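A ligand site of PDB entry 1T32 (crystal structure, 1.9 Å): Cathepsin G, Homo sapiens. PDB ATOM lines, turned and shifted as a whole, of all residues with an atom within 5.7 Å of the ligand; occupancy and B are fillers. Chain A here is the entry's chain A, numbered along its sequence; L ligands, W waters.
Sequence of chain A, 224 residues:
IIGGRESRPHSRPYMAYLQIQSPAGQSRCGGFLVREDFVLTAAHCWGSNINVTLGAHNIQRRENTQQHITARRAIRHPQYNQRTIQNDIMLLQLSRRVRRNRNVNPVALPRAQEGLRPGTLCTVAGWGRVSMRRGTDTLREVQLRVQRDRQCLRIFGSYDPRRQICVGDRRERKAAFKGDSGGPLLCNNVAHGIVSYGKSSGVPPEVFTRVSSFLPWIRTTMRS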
ATOM      1  N   ARG A  28     -10.540  -9.586  -3.853  1.00  0.00           N
ATOM      2  CA  ARG A  28     -10.344  -8.885  -2.579  1.00  0.00           C
ATOM      3  C   ARG A  28     -11.205  -7.637  -2.388  1.00  0.00           C
ATOM      4  O   ARG A  28     -11.342  -6.825  -3.313  1.00  0.00           O
ATOM      5  CB  ARG A  28      -8.862  -8.485  -2.452  1.00  0.00           C
ATOM      6  CG  ARG A  28      -8.570  -7.424  -1.400  1.00  0.00           C
ATOM      7  CD  ARG A  28      -7.152  -6.831  -1.547  1.00  0.00           C
ATOM      8  NE  ARG A  28      -6.130  -7.875  -1.559  1.00  0.00           N
ATOM      9  CZ  ARG A  28      -4.943  -7.786  -0.960  1.00  0.00           C
ATOM     10  NH1 ARG A  28      -4.621  -6.690  -0.280  1.00  0.00           N
ATOM     11  NH2 ARG A  28      -4.085  -8.788  -1.036  1.00  0.00           N
ATOM     12  N   CYS A  29     -11.766  -7.470  -1.186  1.00  0.00           N
ATOM     13  CA  CYS A  29     -12.593  -6.307  -0.857  1.00  0.00           C
ATOM     14  C   CYS A  29     -12.439  -5.909   0.602  1.00  0.00           C
ATOM     15  O   CYS A  29     -11.894  -6.666   1.419  1.00  0.00           O
ATOM     16  CB  CYS A  29     -14.088  -6.587  -1.126  1.00  0.00           C
ATOM     17  SG  CYS A  29     -14.624  -6.319  -2.847  1.00  0.00           S
ATOM     18  N   HIS A  44     -21.170  -5.245  -5.052  1.00  0.00           N
ATOM     19  CA  HIS A  44     -20.439  -5.760  -6.204  1.00  0.00           C
ATOM     20  C   HIS A  44     -19.327  -6.723  -5.758  1.00  0.00           C
ATOM     21  O   HIS A  44     -18.658  -7.340  -6.589  1.00  0.00           O
ATOM     22  CB  HIS A  44     -19.874  -4.618  -7.085  1.00  0.00           C
ATOM     23  CG  HIS A  44     -18.613  -4.000  -6.562  1.00  0.00           C
ATOM     24  ND1 HIS A  44     -18.588  -2.753  -5.960  1.00  0.00           N
ATOM     25  CD2 HIS A  44     -17.337  -4.444  -6.544  1.00  0.00           C
ATOM     26  CE1 HIS A  44     -17.354  -2.463  -5.606  1.00  0.00           C
ATOM     27  NE2 HIS A  44     -16.572  -3.472  -5.936  1.00  0.00           N
ATOM     28  N   CYS A  45     -19.147  -6.855  -4.444  1.00  0.00           N
ATOM     29  CA  CYS A  45     -18.127  -7.765  -3.894  1.00  0.00           C
ATOM     30  C   CYS A  45     -18.752  -9.133  -3.584  1.00  0.00           C
ATOM     31  O   CYS A  45     -18.080 -10.019  -3.052  1.00  0.00           O
ATOM     32  CB  CYS A  45     -17.535  -7.197  -2.595  1.00  0.00           C
ATOM     33  SG  CYS A  45     -16.550  -5.666  -2.699  1.00  0.00           S
ATOM     34  N   TYR A  80     -29.981  -3.773  -5.935  1.00  0.00           N
ATOM     35  CA  TYR A  80     -28.611  -3.621  -6.424  1.00  0.00           C
ATOM     36  C   TYR A  80     -28.602  -3.909  -7.928  1.00  0.00           C
ATOM     37  O   TYR A  80     -29.104  -4.933  -8.374  1.00  0.00           O
ATOM     38  CB  TYR A  80     -27.662  -4.589  -5.719  1.00  0.00           C
ATOM     39  CG  TYR A  80     -26.330  -4.715  -6.408  1.00  0.00           C
ATOM     40  CD1 TYR A  80     -25.504  -3.609  -6.570  1.00  0.00           C
ATOM     41  CD2 TYR A  80     -25.912  -5.932  -6.949  1.00  0.00           C
ATOM     42  CE1 TYR A  80     -24.303  -3.694  -7.261  1.00  0.00           C
ATOM     43  CE2 TYR A  80     -24.712  -6.027  -7.631  1.00  0.00           C
ATOM     44  CZ  TYR A  80     -23.918  -4.914  -7.788  1.00  0.00           C
ATOM     45  OH  TYR A  80     -22.721  -4.995  -8.466  1.00  0.00           O
ATOM     46  N   GLN A  82     -25.953  -4.278 -10.864  1.00  0.00           N
ATOM     47  CA  GLN A  82     -24.543  -4.388 -11.211  1.00  0.00           C
ATOM     48  C   GLN A  82     -24.161  -3.648 -12.488  1.00  0.00           C
ATOM     49  O   GLN A  82     -23.005  -3.292 -12.674  1.00  0.00           O
ATOM     50  CB  GLN A  82     -24.127  -5.857 -11.313  1.00  0.00           C
ATOM     51  CG  GLN A  82     -24.212  -6.472 -12.701  1.00  0.00           C
ATOM     52  CD  GLN A  82     -23.642  -7.885 -12.753  1.00  0.00           C
ATOM     53  OE1 GLN A  82     -23.454  -8.461 -13.827  1.00  0.00           O
ATOM     54  NE2 GLN A  82     -23.366  -8.448 -11.578  1.00  0.00           N
ATOM     55  N   ILE A  85     -24.404  -0.002 -11.205  1.00  0.00           N
ATOM     56  CA  ILE A  85     -23.737   0.047  -9.905  1.00  0.00           C
ATOM     57  C   ILE A  85     -24.517   0.855  -8.876  1.00  0.00           C
ATOM     58  O   ILE A  85     -23.943   1.470  -7.981  1.00  0.00           O
ATOM     59  CB  ILE A  85     -22.304   0.624 -10.006  1.00  0.00           C
ATOM     60  CG1 ILE A  85     -21.584   0.050 -11.229  1.00  0.00           C
ATOM     61  CG2 ILE A  85     -21.495   0.214  -8.770  1.00  0.00           C
ATOM     62  CD1 ILE A  85     -20.195   0.683 -11.479  1.00  0.00           C
ATOM     63  N   ASP A  88     -25.170  -0.086  -4.337  1.00  0.00           N
ATOM     64  CA  ASP A  88     -24.012  -0.937  -4.105  1.00  0.00           C
ATOM     65  C   ASP A  88     -23.763  -1.100  -2.605  1.00  0.00           C
ATOM     66  O   ASP A  88     -22.880  -0.454  -2.021  1.00  0.00           O
ATOM     67  CB  ASP A  88     -22.801  -0.322  -4.809  1.00  0.00           C
ATOM     68  CG  ASP A  88     -21.642  -1.298  -4.960  1.00  0.00           C
ATOM     69  OD1 ASP A  88     -21.850  -2.477  -4.654  1.00  0.00           O
ATOM     70  OD2 ASP A  88     -20.551  -0.873  -5.395  1.00  0.00           O
ATOM     71  N   ILE A 155     -19.702  13.441 -14.450  1.00  0.00           N
ATOM     72  CA  ILE A 155     -18.785  12.354 -14.774  1.00  0.00           C
ATOM     73  C   ILE A 155     -19.391  10.958 -14.830  1.00  0.00           C
ATOM     74  O   ILE A 155     -19.143  10.200 -15.769  1.00  0.00           O
ATOM     75  CB  ILE A 155     -17.605  12.307 -13.761  1.00  0.00           C
ATOM     76  CG1 ILE A 155     -16.876  13.661 -13.766  1.00  0.00           C
ATOM     77  CG2 ILE A 155     -16.647  11.182 -14.110  1.00  0.00           C
ATOM     78  CD1 ILE A 155     -15.818  13.774 -12.686  1.00  0.00           C
ATOM     79  N   PHE A 156     -20.187  10.613 -13.819  1.00  0.00           N
ATOM     80  CA  PHE A 156     -20.790   9.278 -13.723  1.00  0.00           C
ATOM     81  C   PHE A 156     -22.280   9.253 -14.068  1.00  0.00           C
ATOM     82  O   PHE A 156     -23.089   9.928 -13.443  1.00  0.00           O
ATOM     83  CB  PHE A 156     -20.548   8.727 -12.310  1.00  0.00           C
ATOM     84  CG  PHE A 156     -19.090   8.670 -11.930  1.00  0.00           C
ATOM     85  CD1 PHE A 156     -18.237   7.740 -12.535  1.00  0.00           C
ATOM     86  CD2 PHE A 156     -18.555   9.587 -11.029  1.00  0.00           C
ATOM     87  CE1 PHE A 156     -16.865   7.736 -12.230  1.00  0.00           C
ATOM     88  CE2 PHE A 156     -17.187   9.584 -10.734  1.00  0.00           C
ATOM     89  CZ  PHE A 156     -16.342   8.658 -11.334  1.00  0.00           C
ATOM     90  N   GLY A 157     -22.610   8.419 -15.048  1.00  0.00           N
ATOM     91  CA  GLY A 157     -23.977   8.295 -15.528  1.00  0.00           C
ATOM     92  C   GLY A 157     -25.200   8.183 -14.646  1.00  0.00           C
ATOM     93  O   GLY A 157     -26.125   8.981 -14.768  1.00  0.00           O
ATOM     94  N   ALA A 176      -9.670   6.375  -2.757  1.00  0.00           N
ATOM     95  CA  ALA A 176      -9.834   4.946  -2.484  1.00  0.00           C
ATOM     96  C   ALA A 176      -9.645   4.368  -3.890  1.00  0.00           C
ATOM     97  O   ALA A 176      -9.910   5.060  -4.886  1.00  0.00           O
ATOM     98  CB  ALA A 176     -11.240   4.642  -1.979  1.00  0.00           C
ATOM     99  N   PHE A 177      -9.185   3.129  -3.989  1.00  0.00           N
ATOM    100  CA  PHE A 177      -8.941   2.553  -5.298  1.00  0.00           C
ATOM    101  C   PHE A 177      -9.310   1.068  -5.339  1.00  0.00           C
ATOM    102  O   PHE A 177      -9.974   0.566  -4.432  1.00  0.00           O
ATOM    103  CB  PHE A 177      -7.457   2.771  -5.651  1.00  0.00           C
ATOM    104  CG  PHE A 177      -7.122   2.533  -7.094  1.00  0.00           C
ATOM    105  CD1 PHE A 177      -7.990   2.910  -8.111  1.00  0.00           C
ATOM    106  CD2 PHE A 177      -5.905   1.933  -7.438  1.00  0.00           C
ATOM    107  CE1 PHE A 177      -7.656   2.695  -9.461  1.00  0.00           C
ATOM    108  CE2 PHE A 177      -5.564   1.715  -8.770  1.00  0.00           C
ATOM    109  CZ  PHE A 177      -6.439   2.097  -9.782  1.00  0.00           C
ATOM    110  N   LYS A 178      -8.904   0.379  -6.406  1.00  0.00           N
ATOM    111  CA  LYS A 178      -9.218  -1.046  -6.562  1.00  0.00           C
ATOM    112  C   LYS A 178      -8.818  -1.835  -5.321  1.00  0.00           C
ATOM    113  O   LYS A 178      -7.691  -1.724  -4.835  1.00  0.00           O
ATOM    114  CB  LYS A 178      -8.500  -1.597  -7.791  1.00  0.00           C
ATOM    115  CG  LYS A 178      -8.907  -3.035  -8.129  1.00  0.00           C
ATOM    116  CD  LYS A 178      -8.191  -3.529  -9.383  1.00  0.00           C
ATOM    117  CE  LYS A 178      -9.073  -4.478 -10.188  1.00  0.00           C
ATOM    118  NZ  LYS A 178      -9.477  -5.679  -9.422  1.00  0.00           N
ATOM    119  N   GLY A 179      -9.748  -2.630  -4.779  1.00  0.00           N
ATOM    120  CA  GLY A 179      -9.420  -3.397  -3.602  1.00  0.00           C
ATOM    121  C   GLY A 179      -9.902  -2.744  -2.320  1.00  0.00           C
ATOM    122  O   GLY A 179     -10.019  -3.409  -1.293  1.00  0.00           O
ATOM    123  N   ASP A 180     -10.180  -1.441  -2.370  1.00  0.00           N
ATOM    124  CA  ASP A 180     -10.692  -0.715  -1.206  1.00  0.00           C
ATOM    125  C   ASP A 180     -12.224  -0.804  -1.188  1.00  0.00           C
ATOM    126  O   ASP A 180     -12.857  -0.445  -0.202  1.00  0.00           O
ATOM    127  CB  ASP A 180     -10.281   0.750  -1.231  1.00  0.00           C
ATOM    128  CG  ASP A 180      -8.778   0.945  -1.066  1.00  0.00           C
ATOM    129  OD1 ASP A 180      -8.145   0.216  -0.262  1.00  0.00           O
ATOM    130  OD2 ASP A 180      -8.232   1.842  -1.741  1.00  0.00           O
ATOM    131  N   SER A 181     -12.792  -1.271  -2.296  1.00  0.00           N
ATOM    132  CA  SER A 181     -14.237  -1.426  -2.425  1.00  0.00           C
ATOM    133  C   SER A 181     -14.818  -2.066  -1.177  1.00  0.00           C
ATOM    134  O   SER A 181     -14.257  -3.039  -0.653  1.00  0.00           O
ATOM    135  CB  SER A 181     -14.571  -2.319  -3.633  1.00  0.00           C
ATOM    136  OG  SER A 181     -14.060  -1.772  -4.830  1.00  0.00           O
ATOM    137  N   VAL A 195     -16.917   2.355  -0.048  1.00  0.00           N
ATOM    138  CA  VAL A 195     -16.218   2.542  -1.316  1.00  0.00           C
ATOM    139  C   VAL A 195     -16.956   1.736  -2.386  1.00  0.00           C
ATOM    140  O   VAL A 195     -17.160   0.525  -2.229  1.00  0.00           O
ATOM    141  CB  VAL A 195     -14.743   2.061  -1.226  1.00  0.00           C
ATOM    142  CG1 VAL A 195     -14.067   2.156  -2.596  1.00  0.00           C
ATOM    143  CG2 VAL A 195     -14.002   2.904  -0.218  1.00  0.00           C
ATOM    144  N   SER A 196     -17.380   2.406  -3.457  1.00  0.00           N
ATOM    145  CA  SER A 196     -18.116   1.739  -4.519  1.00  0.00           C
ATOM    146  C   SER A 196     -17.303   1.683  -5.818  1.00  0.00           C
ATOM    147  O   SER A 196     -16.904   0.592  -6.255  1.00  0.00           O
ATOM    148  CB  SER A 196     -19.456   2.464  -4.744  1.00  0.00           C
ATOM    149  OG  SER A 196     -20.276   1.768  -5.662  1.00  0.00           O
ATOM    150  N   TYR A 197     -17.055   2.827  -6.446  1.00  0.00           N
ATOM    151  CA  TYR A 197     -16.251   2.831  -7.665  1.00  0.00           C
ATOM    152  C   TYR A 197     -15.773   4.215  -8.074  1.00  0.00           C
ATOM    153  O   TYR A 197     -16.101   5.218  -7.427  1.00  0.00           O
ATOM    154  CB  TYR A 197     -17.021   2.206  -8.838  1.00  0.00           C
ATOM    155  CG  TYR A 197     -18.137   3.054  -9.398  1.00  0.00           C
ATOM    156  CD1 TYR A 197     -19.335   3.207  -8.709  1.00  0.00           C
ATOM    157  CD2 TYR A 197     -17.981   3.709 -10.632  1.00  0.00           C
ATOM    158  CE1 TYR A 197     -20.370   4.002  -9.225  1.00  0.00           C
ATOM    159  CE2 TYR A 197     -19.008   4.499 -11.152  1.00  0.00           C
ATOM    160  CZ  TYR A 197     -20.203   4.641 -10.443  1.00  0.00           C
ATOM    161  OH  TYR A 197     -21.225   5.406 -10.948  1.00  0.00           O
ATOM    162  N   GLY A 198     -15.001   4.253  -9.152  1.00  0.00           N
ATOM    163  CA  GLY A 198     -14.471   5.512  -9.679  1.00  0.00           C
ATOM    164  C   GLY A 198     -13.794   5.196 -10.999  1.00  0.00           C
ATOM    165  O   GLY A 198     -13.951   4.094 -11.510  1.00  0.00           O
ATOM    166  N   LYS A 199     -13.038   6.137 -11.552  1.00  0.00           N
ATOM    167  CA  LYS A 199     -12.349   5.900 -12.822  1.00  0.00           C
ATOM    168  C   LYS A 199     -11.248   4.846 -12.627  1.00  0.00           C
ATOM    169  O   LYS A 199     -10.659   4.753 -11.544  1.00  0.00           O
ATOM    170  CB  LYS A 199     -11.740   7.206 -13.355  1.00  0.00           C
ATOM    171  CG  LYS A 199     -12.790   8.278 -13.647  1.00  0.00           C
ATOM    172  CD  LYS A 199     -12.199   9.505 -14.361  1.00  0.00           C
ATOM    173  CE  LYS A 199     -11.172  10.215 -13.488  1.00  0.00           C
ATOM    174  NZ  LYS A 199     -10.781  11.551 -14.052  1.00  0.00           N
ATOM    175  N   SER A 200     -10.962   4.067 -13.664  1.00  0.00           N
ATOM    176  CA  SER A 200      -9.935   3.023 -13.545  1.00  0.00           C
ATOM    177  C   SER A 200      -8.552   3.611 -13.292  1.00  0.00           C
ATOM    178  O   SER A 200      -7.641   2.888 -12.875  1.00  0.00           O
ATOM    179  CB  SER A 200      -9.923   2.136 -14.796  1.00  0.00           C
ATOM    180  OG  SER A 200      -9.550   2.860 -15.950  1.00  0.00           O
ATOM    181  N   GLY A 202      -8.062   5.960 -11.100  1.00  0.00           N
ATOM    182  CA  GLY A 202      -8.003   6.281  -9.677  1.00  0.00           C
ATOM    183  C   GLY A 202      -8.029   7.775  -9.414  1.00  0.00           C
ATOM    184  O   GLY A 202      -7.914   8.218  -8.274  1.00  0.00           O
ATOM    185  N   GLU A 206     -14.647  10.318  -7.009  1.00  0.00           N
ATOM    186  CA  GLU A 206     -15.041   8.906  -7.040  1.00  0.00           C
ATOM    187  C   GLU A 206     -16.374   8.783  -6.298  1.00  0.00           C
ATOM    188  O   GLU A 206     -16.804   9.711  -5.606  1.00  0.00           O
ATOM    189  CB  GLU A 206     -13.958   8.014  -6.416  1.00  0.00           C
ATOM    190  CG  GLU A 206     -13.572   8.355  -4.991  1.00  0.00           C
ATOM    191  CD  GLU A 206     -12.415   7.512  -4.482  1.00  0.00           C
ATOM    192  OE1 GLU A 206     -11.851   6.739  -5.277  1.00  0.00           O
ATOM    193  OE2 GLU A 206     -12.067   7.618  -3.285  1.00  0.00           O
ATOM    194  N   VAL A 207     -17.018   7.630  -6.445  1.00  0.00           N
ATOM    195  CA  VAL A 207     -18.330   7.398  -5.850  1.00  0.00           C
ATOM    196  C   VAL A 207     -18.353   6.441  -4.665  1.00  0.00           C
ATOM    197  O   VAL A 207     -17.743   5.378  -4.695  1.00  0.00           O
ATOM    198  CB  VAL A 207     -19.299   6.864  -6.921  1.00  0.00           C
ATOM    199  CG1 VAL A 207     -20.665   6.582  -6.320  1.00  0.00           C
ATOM    200  CG2 VAL A 207     -19.426   7.878  -8.063  1.00  0.00           C
HETATM  201  O1  LIG L   1     -17.551  -0.242 -14.638  1.00  0.00           O
HETATM  202  P1  LIG L   1     -12.836  -3.940  -7.030  1.00  0.00           P
HETATM  203  O2  LIG L   1     -11.690  -4.986  -7.362  1.00  0.00           O
HETATM  204  O3  LIG L   1     -12.136  -2.974  -6.074  1.00  0.00           O
HETATM  205  O4  LIG L   1     -13.967  -4.613  -6.326  1.00  0.00           O
HETATM  206  C1  LIG L   1     -13.530  -2.963  -8.312  1.00  0.00           C
HETATM  207  O5  LIG L   1     -11.661  -2.837  -9.800  1.00  0.00           O
HETATM  208  C2  LIG L   1     -12.397  -2.259  -9.045  1.00  0.00           C
HETATM  209  C3  LIG L   1     -13.048   2.067  -6.255  1.00  0.00           C
HETATM  210  C4  LIG L   1     -12.872   3.502  -6.102  1.00  0.00           C
HETATM  211  C5  LIG L   1     -12.169   4.280  -7.141  1.00  0.00           C
HETATM  212  C6  LIG L   1     -11.622   3.691  -8.355  1.00  0.00           C
HETATM  213  C7  LIG L   1     -11.776   2.227  -8.555  1.00  0.00           C
HETATM  214  C8  LIG L   1     -12.539   1.350  -7.460  1.00  0.00           C
HETATM  215  C9  LIG L   1     -12.719  -0.083  -7.622  1.00  0.00           C
HETATM  216  C10 LIG L   1     -12.199  -0.738  -8.833  1.00  0.00           C
HETATM  217  C11 LIG L   1     -11.460   0.072  -9.917  1.00  0.00           C
HETATM  218  C12 LIG L   1     -11.269   1.535  -9.744  1.00  0.00           C
HETATM  219  O6  LIG L   1      -9.622  -0.637 -11.249  1.00  0.00           O
HETATM  220  C13 LIG L   1     -10.845  -0.443 -11.261  1.00  0.00           C
HETATM  221  C14 LIG L   1     -16.341  -5.213 -11.232  1.00  0.00           C
HETATM  222  C15 LIG L   1     -15.011  -5.742 -11.062  1.00  0.00           C
HETATM  223  C16 LIG L   1     -14.019  -5.097 -10.129  1.00  0.00           C
HETATM  224  C17 LIG L   1     -14.302  -3.860  -9.336  1.00  0.00           C
HETATM  225  C18 LIG L   1     -15.772  -3.215  -9.492  1.00  0.00           C
HETATM  226  C19 LIG L   1     -16.793  -4.017 -10.535  1.00  0.00           C
HETATM  227  C20 LIG L   1     -18.191  -3.501 -10.742  1.00  0.00           C
HETATM  228  C21 LIG L   1     -18.672  -2.313 -10.067  1.00  0.00           C
HETATM  229  C22 LIG L   1     -17.774  -1.543  -9.117  1.00  0.00           C
HETATM  230  C23 LIG L   1     -16.383  -2.004  -8.866  1.00  0.00           C
HETATM  231  N1  LIG L   1     -11.706  -0.631 -12.418  1.00  0.00           N
HETATM  232  C24 LIG L   1     -11.124  -1.111 -13.719  1.00  0.00           C
HETATM  233  C25 LIG L   1     -15.182   1.335 -12.249  1.00  0.00           C
HETATM  234  N2  LIG L   1     -15.942   0.290 -13.079  1.00  0.00           N
HETATM  235  C26 LIG L   1     -15.644  -1.160 -12.673  1.00  0.00           C
HETATM  236  C27 LIG L   1     -14.092  -1.426 -12.862  1.00  0.00           C
HETATM  237  C28 LIG L   1     -13.232  -0.279 -12.161  1.00  0.00           C
HETATM  238  C29 LIG L   1     -13.677   1.147 -12.594  1.00  0.00           C
HETATM  239  C30 LIG L   1     -16.877   0.659 -14.088  1.00  0.00           C
HETATM  240  C31 LIG L   1     -18.851   4.027 -15.013  1.00  0.00           C
HETATM  241  C32 LIG L   1     -18.537   2.651 -14.593  1.00  0.00           C
HETATM  242  C33 LIG L   1     -17.127   2.144 -14.544  1.00  0.00           C
HETATM  243  C34 LIG L   1     -16.016   3.085 -14.923  1.00  0.00           C
HETATM  244  C35 LIG L   1     -16.276   4.431 -15.329  1.00  0.00           C
HETATM  245  C36 LIG L   1     -17.771   4.941 -15.372  1.00  0.00           C
HETATM  246  C37 LIG L   1     -18.024   6.318 -15.776  1.00  0.00           C
HETATM  247  C38 LIG L   1     -16.891   7.191 -16.131  1.00  0.00           C
HETATM  248  C39 LIG L   1     -15.495   6.714 -16.094  1.00  0.00           C
HETATM  249  C40 LIG L   1     -15.184   5.350 -15.692  1.00  0.00           C
HETATM  250  O   HOH W   1      -9.958  -6.040  -5.659  1.00  0.00           O
HETATM  251  O   HOH W   2     -11.955   5.253 -16.184  1.00  0.00           O
HETATM  252  O   HOH W   3      -7.496   0.156 -12.809  1.00  0.00           O
HETATM  253  O   HOH W   4     -15.049   5.240  -4.269  1.00  0.00           O
HETATM  254  O   HOH W   5     -15.005  -6.968  -7.235  1.00  0.00           O
HETATM  255  O   HOH W   6     -12.481  -7.764  -8.498  1.00  0.00           O
HETATM  256  O   HOH W   7     -21.474   1.062 -15.338  1.00  0.00           O
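O4 of the ligand sits at hydrogen-bond distance from NE2 of His 44. The backbone NH (N) of Gly 179 is in hydrogen-bond range of an oxygen (O3) of the ligand. OG of Ser 181 sits at hydrogen-bond distance from O3 of the ligand (2.6 Å). NZ of Lys 178 is in salt-bridge range of O2 of the ligand, at 3.1 Å.
A ring nitrogen (NE2) of His 44 lies within hydrogen-bond range of the side-chain hydroxyl (OG) of Ser 181 (3.2 Å). The side-chain carboxylate of Asp 88 is in hydrogen-bond range of a ring nitrogen (ND1) of His 44 (2.8 Å). The side-chain sulfur of Cys 45 forms a disulfide with the side-chain sulfur of Cys 29 (2.0 Å). The backbone NH (N) of Phe 177 is in hydrogen-bond range of the side-chain carboxylate (OD2) of Asp 180 (2.8 Å). The backbone NH of Ala 176 is in hydrogen-bond range of the side-chain carboxylate of Glu 206 (2.8 Å). The backbone NH (N) of Ser 196 is in hydrogen-bond range of the backbone carbonyl oxygen (O) of Val 207 (3.2 Å). The side-chain carboxylate of Asp 88 lies within hydrogen-bond range of the side-chain hydroxyl of Ser 196 (2.7 Å). The backbone NH (N) of Val 207 sits at hydrogen-bond distance from the backbone carbonyl oxygen (O) of Tyr 197, 2.8 Å away.
Residues that only touch the ligand: Cys 29, Ile 85, Ile 155, Phe 156, Ala 176, Phe 177, Val 195, Ser 196, Tyr 197, Gly 198, Lys 199, Ser 200 and Glu 206. Hydrophobic or aromatic side chains within 4 Å of the ligand: His 44, Ile 85, Phe 156, Phe 177, Val 195 and Tyr 197.
Water W1 bridges O2 of the ligand (2.6 Å) and O of Arg 28 (2.8 Å). Water W3 bridges O of Ser 200 (2.7 Å) and O6 of the ligand (2.8 Å). Water W4 bridges O of Val 207 (2.7 Å) and O of Tyr 197 (3.3 Å).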
